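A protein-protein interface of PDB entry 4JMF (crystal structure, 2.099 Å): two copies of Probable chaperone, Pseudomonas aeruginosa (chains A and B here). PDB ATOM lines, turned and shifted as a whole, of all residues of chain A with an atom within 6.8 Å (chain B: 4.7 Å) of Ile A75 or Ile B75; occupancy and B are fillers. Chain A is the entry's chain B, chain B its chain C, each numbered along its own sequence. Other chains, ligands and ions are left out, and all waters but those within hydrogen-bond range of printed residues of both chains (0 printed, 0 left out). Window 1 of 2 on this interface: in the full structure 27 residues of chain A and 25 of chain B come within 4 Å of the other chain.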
ATOM      1  N   GLN A  64      20.909 -14.963  -2.391  1.00  0.00           N
ATOM      2  CA  GLN A  64      19.799 -15.643  -1.736  1.00  0.00           C
ATOM      3  C   GLN A  64      18.507 -14.842  -1.909  1.00  0.00           C
ATOM      4  O   GLN A  64      17.420 -15.415  -2.048  1.00  0.00           O
ATOM      5  CB  GLN A  64      20.099 -15.848  -0.250  1.00  0.00           C
ATOM      6  CG  GLN A  64      19.034 -16.680   0.470  1.00  0.00           C
ATOM      7  CD  GLN A  64      18.957 -18.095  -0.073  1.00  0.00           C
ATOM      8  OE1 GLN A  64      19.954 -18.818  -0.093  1.00  0.00           O
ATOM      9  NE2 GLN A  64      17.769 -18.496  -0.535  1.00  0.00           N
ATOM     10  N   ASN A  65      18.636 -13.517  -1.932  1.00  0.00           N
ATOM     11  CA  ASN A  65      17.467 -12.638  -2.015  1.00  0.00           C
ATOM     12  C   ASN A  65      17.073 -12.211  -3.432  1.00  0.00           C
ATOM     13  O   ASN A  65      16.226 -11.322  -3.628  1.00  0.00           O
ATOM     14  CB  ASN A  65      17.646 -11.442  -1.074  1.00  0.00           C
ATOM     15  CG  ASN A  65      17.617 -11.868   0.386  1.00  0.00           C
ATOM     16  OD1 ASN A  65      16.901 -12.803   0.742  1.00  0.00           O
ATOM     17  ND2 ASN A  65      18.417 -11.216   1.225  1.00  0.00           N
ATOM     18  N   LEU A  66      17.686 -12.858  -4.416  1.00  0.00           N
ATOM     19  CA  LEU A  66      17.282 -12.700  -5.811  1.00  0.00           C
ATOM     20  C   LEU A  66      16.292 -13.805  -6.171  1.00  0.00           C
ATOM     21  O   LEU A  66      16.429 -14.953  -5.723  1.00  0.00           O
ATOM     22  CB  LEU A  66      18.499 -12.805  -6.731  1.00  0.00           C
ATOM     23  CG  LEU A  66      18.249 -12.533  -8.212  1.00  0.00           C
ATOM     24  CD1 LEU A  66      17.651 -11.146  -8.361  1.00  0.00           C
ATOM     25  CD2 LEU A  66      19.547 -12.650  -8.992  1.00  0.00           C
ATOM     26  N   PHE A  67      15.290 -13.460  -6.967  1.00  0.00           N
ATOM     27  CA  PHE A  67      14.299 -14.440  -7.400  1.00  0.00           C
ATOM     28  C   PHE A  67      14.957 -15.538  -8.245  1.00  0.00           C
ATOM     29  O   PHE A  67      15.973 -15.296  -8.901  1.00  0.00           O
ATOM     30  CB  PHE A  67      13.187 -13.747  -8.199  1.00  0.00           C
ATOM     31  CG  PHE A  67      13.679 -13.011  -9.416  1.00  0.00           C
ATOM     32  CD1 PHE A  67      13.897 -11.632  -9.375  1.00  0.00           C
ATOM     33  CD2 PHE A  67      13.917 -13.690 -10.605  1.00  0.00           C
ATOM     34  CE1 PHE A  67      14.347 -10.945 -10.505  1.00  0.00           C
ATOM     35  CE2 PHE A  67      14.377 -13.011 -11.738  1.00  0.00           C
ATOM     36  CZ  PHE A  67      14.585 -11.639 -11.685  1.00  0.00           C
ATOM     37  N   PRO A  71       9.228 -20.063  -6.743  1.00  0.00           N
ATOM     38  CA  PRO A  71       8.688 -19.083  -5.785  1.00  0.00           C
ATOM     39  C   PRO A  71       8.890 -19.457  -4.311  1.00  0.00           C
ATOM     40  O   PRO A  71       8.778 -18.566  -3.451  1.00  0.00           O
ATOM     41  CB  PRO A  71       7.184 -19.062  -6.109  1.00  0.00           C
ATOM     42  CG  PRO A  71       7.098 -19.563  -7.531  1.00  0.00           C
ATOM     43  CD  PRO A  71       8.180 -20.604  -7.627  1.00  0.00           C
ATOM     44  N   CYS A  72       9.193 -20.723  -4.014  1.00  0.00           N
ATOM     45  CA  CYS A  72       9.428 -21.118  -2.625  1.00  0.00           C
ATOM     46  C   CYS A  72      10.874 -20.910  -2.187  1.00  0.00           C
ATOM     47  O   CYS A  72      11.231 -21.240  -1.046  1.00  0.00           O
ATOM     48  CB  CYS A  72       9.031 -22.581  -2.398  1.00  0.00           C
ATOM     49  SG  CYS A  72       7.252 -22.875  -2.574  1.00  0.00           S
ATOM     50  N   LYS A  73      11.717 -20.401  -3.084  1.00  0.00           N
ATOM     51  CA  LYS A  73      13.104 -20.094  -2.689  1.00  0.00           C
ATOM     52  C   LYS A  73      12.991 -19.067  -1.576  1.00  0.00           C
ATOM     53  O   LYS A  73      12.304 -18.052  -1.736  1.00  0.00           O
ATOM     54  CB  LYS A  73      13.907 -19.506  -3.844  1.00  0.00           C
ATOM     55  CG  LYS A  73      15.316 -19.069  -3.426  1.00  0.00           C
ATOM     56  CD  LYS A  73      16.012 -18.312  -4.538  1.00  0.00           C
ATOM     57  CE  LYS A  73      17.432 -17.920  -4.106  1.00  0.00           C
ATOM     58  NZ  LYS A  73      18.171 -17.208  -5.187  1.00  0.00           N
ATOM     59  N   PRO A  74      13.608 -19.348  -0.422  1.00  0.00           N
ATOM     60  CA  PRO A  74      13.365 -18.457   0.716  1.00  0.00           C
ATOM     61  C   PRO A  74      14.166 -17.161   0.647  1.00  0.00           C
ATOM     62  O   PRO A  74      15.113 -17.021  -0.134  1.00  0.00           O
ATOM     63  CB  PRO A  74      13.809 -19.294   1.923  1.00  0.00           C
ATOM     64  CG  PRO A  74      14.815 -20.242   1.360  1.00  0.00           C
ATOM     65  CD  PRO A  74      14.452 -20.501  -0.067  1.00  0.00           C
ATOM     66  N   ILE A  75      13.763 -16.219   1.492  1.00  0.00           N
ATOM     67  CA  ILE A  75      14.324 -14.886   1.522  1.00  0.00           C
ATOM     68  C   ILE A  75      14.985 -14.737   2.890  1.00  0.00           C
ATOM     69  O   ILE A  75      14.494 -15.298   3.866  1.00  0.00           O
ATOM     70  CB  ILE A  75      13.184 -13.858   1.409  1.00  0.00           C
ATOM     71  CG1 ILE A  75      12.350 -14.131   0.164  1.00  0.00           C
ATOM     72  CG2 ILE A  75      13.706 -12.422   1.430  1.00  0.00           C
ATOM     73  CD1 ILE A  75      13.150 -14.174  -1.074  1.00  0.00           C
ATOM     74  N   LEU A  76      16.089 -13.995   2.977  1.00  0.00           N
ATOM     75  CA  LEU A  76      16.742 -13.788   4.271  1.00  0.00           C
ATOM     76  C   LEU A  76      16.649 -12.323   4.676  1.00  0.00           C
ATOM     77  O   LEU A  76      17.246 -11.455   4.040  1.00  0.00           O
ATOM     78  CB  LEU A  76      18.206 -14.233   4.229  1.00  0.00           C
ATOM     79  CG  LEU A  76      18.977 -14.135   5.546  1.00  0.00           C
ATOM     80  CD1 LEU A  76      18.189 -14.829   6.639  1.00  0.00           C
ATOM     81  CD2 LEU A  76      20.341 -14.772   5.423  1.00  0.00           C
ATOM     82  N   GLY A  77      15.891 -12.047   5.727  1.00  0.00           N
ATOM     83  CA  GLY A  77      15.647 -10.675   6.136  1.00  0.00           C
ATOM     84  C   GLY A  77      15.869 -10.514   7.627  1.00  0.00           C
ATOM     85  O   GLY A  77      16.278 -11.461   8.317  1.00  0.00           O
ATOM     86  N   LEU A  86      15.769 -13.790   9.966  1.00  0.00           N
ATOM     87  CA  LEU A  86      14.800 -14.852   9.669  1.00  0.00           C
ATOM     88  C   LEU A  86      14.860 -15.228   8.196  1.00  0.00           C
ATOM     89  O   LEU A  86      14.780 -14.355   7.314  1.00  0.00           O
ATOM     90  CB  LEU A  86      13.379 -14.404  10.030  1.00  0.00           C
ATOM     91  CG  LEU A  86      13.073 -13.915  11.450  1.00  0.00           C
ATOM     92  CD1 LEU A  86      11.596 -13.572  11.586  1.00  0.00           C
ATOM     93  CD2 LEU A  86      13.466 -14.952  12.501  1.00  0.00           C
ATOM     94  N   LEU A  87      15.026 -16.522   7.932  1.00  0.00           N
ATOM     95  CA  LEU A  87      14.958 -17.064   6.572  1.00  0.00           C
ATOM     96  C   LEU A  87      13.509 -17.532   6.385  1.00  0.00           C
ATOM     97  O   LEU A  87      13.001 -18.277   7.211  1.00  0.00           O
ATOM     98  CB  LEU A  87      15.917 -18.251   6.457  1.00  0.00           C
ATOM     99  CG  LEU A  87      16.089 -18.949   5.119  1.00  0.00           C
ATOM    100  CD1 LEU A  87      16.828 -18.024   4.188  1.00  0.00           C
ATOM    101  CD2 LEU A  87      16.858 -20.257   5.294  1.00  0.00           C
ATOM    102  N   TRP A  88      12.834 -17.088   5.326  1.00  0.00           N
ATOM    103  CA  TRP A  88      11.394 -17.314   5.226  1.00  0.00           C
ATOM    104  C   TRP A  88      10.923 -17.489   3.806  1.00  0.00           C
ATOM    105  O   TRP A  88      11.547 -16.995   2.855  1.00  0.00           O
ATOM    106  CB  TRP A  88      10.618 -16.145   5.844  1.00  0.00           C
ATOM    107  CG  TRP A  88      10.859 -14.830   5.147  1.00  0.00           C
ATOM    108  CD1 TRP A  88      11.899 -13.966   5.365  1.00  0.00           C
ATOM    109  CD2 TRP A  88      10.050 -14.231   4.121  1.00  0.00           C
ATOM    110  NE1 TRP A  88      11.781 -12.861   4.550  1.00  0.00           N
ATOM    111  CE2 TRP A  88      10.658 -13.002   3.771  1.00  0.00           C
ATOM    112  CE3 TRP A  88       8.870 -14.611   3.464  1.00  0.00           C
ATOM    113  CZ2 TRP A  88      10.127 -12.151   2.795  1.00  0.00           C
ATOM    114  CZ3 TRP A  88       8.338 -13.760   2.493  1.00  0.00           C
ATOM    115  CH2 TRP A  88       8.969 -12.541   2.170  1.00  0.00           C
ATOM    116  N   ASN A  89       9.800 -18.188   3.658  1.00  0.00           N
ATOM    117  CA  ASN A  89       9.098 -18.166   2.379  1.00  0.00           C
ATOM    118  C   ASN A  89       7.596 -18.144   2.614  1.00  0.00           C
ATOM    119  O   ASN A  89       7.149 -18.229   3.761  1.00  0.00           O
ATOM    120  CB  ASN A  89       9.565 -19.286   1.441  1.00  0.00           C
ATOM    121  CG  ASN A  89       9.335 -20.676   2.011  1.00  0.00           C
ATOM    122  OD1 ASN A  89       8.554 -20.867   2.955  1.00  0.00           O
ATOM    123  ND2 ASN A  89      10.008 -21.664   1.423  1.00  0.00           N
ATOM    124  N   LEU A 108      12.776 -24.239   2.091  1.00  0.00           N
ATOM    125  CA  LEU A 108      13.205 -23.474   3.261  1.00  0.00           C
ATOM    126  C   LEU A 108      14.391 -24.177   3.912  1.00  0.00           C
ATOM    127  O   LEU A 108      15.457 -23.580   4.111  1.00  0.00           O
ATOM    128  CB  LEU A 108      12.071 -23.335   4.283  1.00  0.00           C
ATOM    129  CG  LEU A 108      12.451 -22.548   5.542  1.00  0.00           C
ATOM    130  CD1 LEU A 108      12.855 -21.109   5.191  1.00  0.00           C
ATOM    131  CD2 LEU A 108      11.320 -22.560   6.576  1.00  0.00           C
ATOM    132  N   ASN B  65      14.121  -6.827   3.315  1.00  0.00           N
ATOM    133  CA  ASN B  65      14.027  -8.243   2.977  1.00  0.00           C
ATOM    134  C   ASN B  65      13.303  -9.088   4.015  1.00  0.00           C
ATOM    135  O   ASN B  65      13.269 -10.314   3.891  1.00  0.00           O
ATOM    136  CB  ASN B  65      15.415  -8.822   2.687  1.00  0.00           C
ATOM    137  CG  ASN B  65      15.989  -8.308   1.386  1.00  0.00           C
ATOM    138  OD1 ASN B  65      15.241  -7.862   0.511  1.00  0.00           O
ATOM    139  ND2 ASN B  65      17.321  -8.369   1.241  1.00  0.00           N
ATOM    140  N   LYS B  73       5.350  -6.729  -0.924  1.00  0.00           N
ATOM    141  CA  LYS B  73       6.497  -5.941  -0.463  1.00  0.00           C
ATOM    142  C   LYS B  73       7.733  -6.400  -1.222  1.00  0.00           C
ATOM    143  O   LYS B  73       8.054  -7.593  -1.223  1.00  0.00           O
ATOM    144  CB  LYS B  73       6.720  -6.099   1.046  1.00  0.00           C
ATOM    145  CG  LYS B  73       7.896  -5.280   1.550  1.00  0.00           C
ATOM    146  CD  LYS B  73       8.210  -5.543   3.018  1.00  0.00           C
ATOM    147  CE  LYS B  73       9.459  -4.753   3.426  1.00  0.00           C
ATOM    148  NZ  LYS B  73       9.968  -5.116   4.788  1.00  0.00           N
ATOM    149  N   PRO B  74       8.410  -5.461  -1.909  1.00  0.00           N
ATOM    150  CA  PRO B  74       9.553  -5.857  -2.732  1.00  0.00           C
ATOM    151  C   PRO B  74      10.710  -6.411  -1.917  1.00  0.00           C
ATOM    152  O   PRO B  74      10.868  -6.108  -0.725  1.00  0.00           O
ATOM    153  CB  PRO B  74       9.967  -4.546  -3.423  1.00  0.00           C
ATOM    154  CG  PRO B  74       8.728  -3.717  -3.427  1.00  0.00           C
ATOM    155  CD  PRO B  74       8.044  -4.044  -2.121  1.00  0.00           C
ATOM    156  N   ILE B  75      11.515  -7.224  -2.592  1.00  0.00           N
ATOM    157  CA  ILE B  75      12.678  -7.870  -2.015  1.00  0.00           C
ATOM    158  C   ILE B  75      13.897  -7.341  -2.779  1.00  0.00           C
ATOM    159  O   ILE B  75      13.803  -7.086  -3.988  1.00  0.00           O
ATOM    160  CB  ILE B  75      12.523  -9.411  -2.125  1.00  0.00           C
ATOM    161  CG1 ILE B  75      11.375  -9.858  -1.195  1.00  0.00           C
ATOM    162  CG2 ILE B  75      13.839 -10.147  -1.792  1.00  0.00           C
ATOM    163  CD1 ILE B  75      10.965 -11.277  -1.354  1.00  0.00           C
ATOM    164  N   LEU B  76      15.016  -7.127  -2.079  1.00  0.00           N
ATOM    165  CA  LEU B  76      16.213  -6.551  -2.698  1.00  0.00           C
ATOM    166  C   LEU B  76      17.294  -7.614  -2.826  1.00  0.00           C
ATOM    167  O   LEU B  76      17.832  -8.085  -1.822  1.00  0.00           O
ATOM    168  CB  LEU B  76      16.731  -5.346  -1.898  1.00  0.00           C
ATOM    169  CG  LEU B  76      17.994  -4.626  -2.432  1.00  0.00           C
ATOM    170  CD1 LEU B  76      17.911  -4.390  -3.927  1.00  0.00           C
ATOM    171  CD2 LEU B  76      18.242  -3.290  -1.731  1.00  0.00           C
ATOM    172  N   GLY B  77      17.600  -8.006  -4.061  1.00  0.00           N
ATOM    173  CA  GLY B  77      18.585  -9.041  -4.298  1.00  0.00           C
ATOM    174  C   GLY B  77      19.742  -8.569  -5.162  1.00  0.00           C
ATOM    175  O   GLY B  77      19.801  -7.398  -5.544  1.00  0.00           O
ATOM    176  N   LEU B  86      18.847  -5.805  -7.734  1.00  0.00           N
ATOM    177  CA  LEU B  86      17.504  -5.786  -8.295  1.00  0.00           C
ATOM    178  C   LEU B  86      16.463  -5.806  -7.194  1.00  0.00           C
ATOM    179  O   LEU B  86      16.524  -6.626  -6.270  1.00  0.00           O
ATOM    180  CB  LEU B  86      17.302  -6.989  -9.223  1.00  0.00           C
ATOM    181  CG  LEU B  86      18.368  -7.052 -10.317  1.00  0.00           C
ATOM    182  CD1 LEU B  86      18.800  -8.475 -10.589  1.00  0.00           C
ATOM    183  CD2 LEU B  86      17.857  -6.373 -11.581  1.00  0.00           C
ATOM    184  N   LEU B  87      15.505  -4.896  -7.293  1.00  0.00           N
ATOM    185  CA  LEU B  87      14.379  -4.878  -6.384  1.00  0.00           C
ATOM    186  C   LEU B  87      13.248  -5.577  -7.141  1.00  0.00           C
ATOM    187  O   LEU B  87      13.054  -5.322  -8.333  1.00  0.00           O
ATOM    188  CB  LEU B  87      14.039  -3.428  -6.071  1.00  0.00           C
ATOM    189  CG  LEU B  87      13.153  -3.132  -4.875  1.00  0.00           C
ATOM    190  CD1 LEU B  87      13.880  -3.398  -3.569  1.00  0.00           C
ATOM    191  CD2 LEU B  87      12.704  -1.682  -4.955  1.00  0.00           C
ATOM    192  N   TRP B  88      12.530  -6.479  -6.476  1.00  0.00           N
ATOM    193  CA  TRP B  88      11.551  -7.305  -7.170  1.00  0.00           C
ATOM    194  C   TRP B  88      10.403  -7.747  -6.282  1.00  0.00           C
ATOM    195  O   TRP B  88      10.539  -7.850  -5.044  1.00  0.00           O
ATOM    196  CB  TRP B  88      12.231  -8.541  -7.781  1.00  0.00           C
ATOM    197  CG  TRP B  88      12.796  -9.501  -6.773  1.00  0.00           C
ATOM    198  CD1 TRP B  88      14.041  -9.453  -6.199  1.00  0.00           C
ATOM    199  CD2 TRP B  88      12.159 -10.676  -6.242  1.00  0.00           C
ATOM    200  NE1 TRP B  88      14.210 -10.521  -5.339  1.00  0.00           N
ATOM    201  CE2 TRP B  88      13.072 -11.283  -5.349  1.00  0.00           C
ATOM    202  CE3 TRP B  88      10.900 -11.266  -6.428  1.00  0.00           C
ATOM    203  CZ2 TRP B  88      12.765 -12.449  -4.633  1.00  0.00           C
ATOM    204  CZ3 TRP B  88      10.592 -12.431  -5.719  1.00  0.00           C
ATOM    205  CH2 TRP B  88      11.522 -13.010  -4.834  1.00  0.00           C
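ND2 of Asn A65 sits close to ND2 of Asn B65 (3.1 Å).
The backbone carbonyl oxygen of Asn A65 lies within hydrogen-bond range of the indole nitrogen of Trp B88 (2.8 Å).
The indole nitrogen of Trp A88 lies within hydrogen-bond range of the backbone carbonyl oxygen of Asn B65.
Of chain B, only Asn B65 (3.3 Å), Ile B75 (3.5 Å) and Trp B88 (3.97 Å) come within 4 Å of Ile A75.
Ile B75 touches two residues of chain A.
Of the printed residues of chain B, Asn A65 touches Asn B65 (3.1 Å), Ile B75 (3.2 Å), Leu B76 (3.4 Å), Gly B77 (3.3 Å) and Trp B88 (2.8 Å).
Of the printed residues of chain A, Leu B86 touches Leu A66.
Of the printed residues of chain B, Trp A88 touches Asn B65.
The nearest printed residue of chain B that does not touch Ile A75 is Leu B76 (6.5 Å).
The nearest residue of chain A that does not touch Ile B75 is Trp A88 (4.2 Å).
Of the 9 printed residues of chain B, 6 touch a printed residue of chain A.
Printed residues of chain B that touch a printed residue of chain A: Asn B65, Ile B75, Leu B76, Gly B77, Leu B86 and Trp B88.
Of the 16 printed residues of chain A, 7 touch a printed residue of chain B.
Hydrophobic or aromatic side chains of chain A within 4 Å of the printed part of chain B: Leu A66, Phe A67, Ile A75 and Trp A88.
Among the printed residues, no Asp or Glu carboxylate lies within 4 Å of a Lys or Arg side-chain nitrogen of the other chain.
Among the printed residues, merely in contact across the chains: Asn A65 with Ile B75 (3.2 Å), Ile A75 with Asn B65 (3.3 Å), Gly A77 with Asn B65 (3.3 Å), Asn A65 with Gly B77 (3.3 Å), Asn A65 with Leu B76 (3.4 Å), Leu A76 with Asn B65 (3.5 Å), Phe A67 with Trp B88 (3.5 Å), Ile A75 with Ile B75 (3.5 Å), Leu A66 with Leu B86 (3.7 Å), Leu A66 with Trp B88 (3.8 Å), Leu A66 with Gly B77 (3.9 Å) and Ile A75 with Trp B88 (3.97 Å).
O of Leu A66 sits at hydrogen-bond distance from NZ of Lys A73, at 2.9 Å.
The backbone NH of Gly B77 sits at hydrogen-bond distance from the backbone carbonyl oxygen of Leu B86 (2.8 Å).
O of Trp B88 sits at hydrogen-bond distance from N of Ile B75, 2.7 Å away.
O of Gly A77 sits at hydrogen-bond distance from N of Leu A86 (2.9 Å).
The side-chain amide oxygen (OD1) of Asn B65 is in hydrogen-bond range of the backbone NH (N) of Leu B76 (2.7 Å).
OD1 of Asn A65 lies within hydrogen-bond range of N of Leu A76 (2.7 Å).
Asn A65 touches Leu B76, and with the chains exchanged Leu A76 touches Asn B65.
Asn A65 touches Gly B77, and with the chains exchanged Gly A77 touches Asn B65.
Ile A75 touches its own counterpart, Ile B75.
Ile A75 touches Trp B88, but with the chains exchanged Trp A88 does not touch Ile B75 (4.2 Å).
Positions printed for both chains: 65, 73, 74, 75, 76, 77, 86, 87 and 88.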
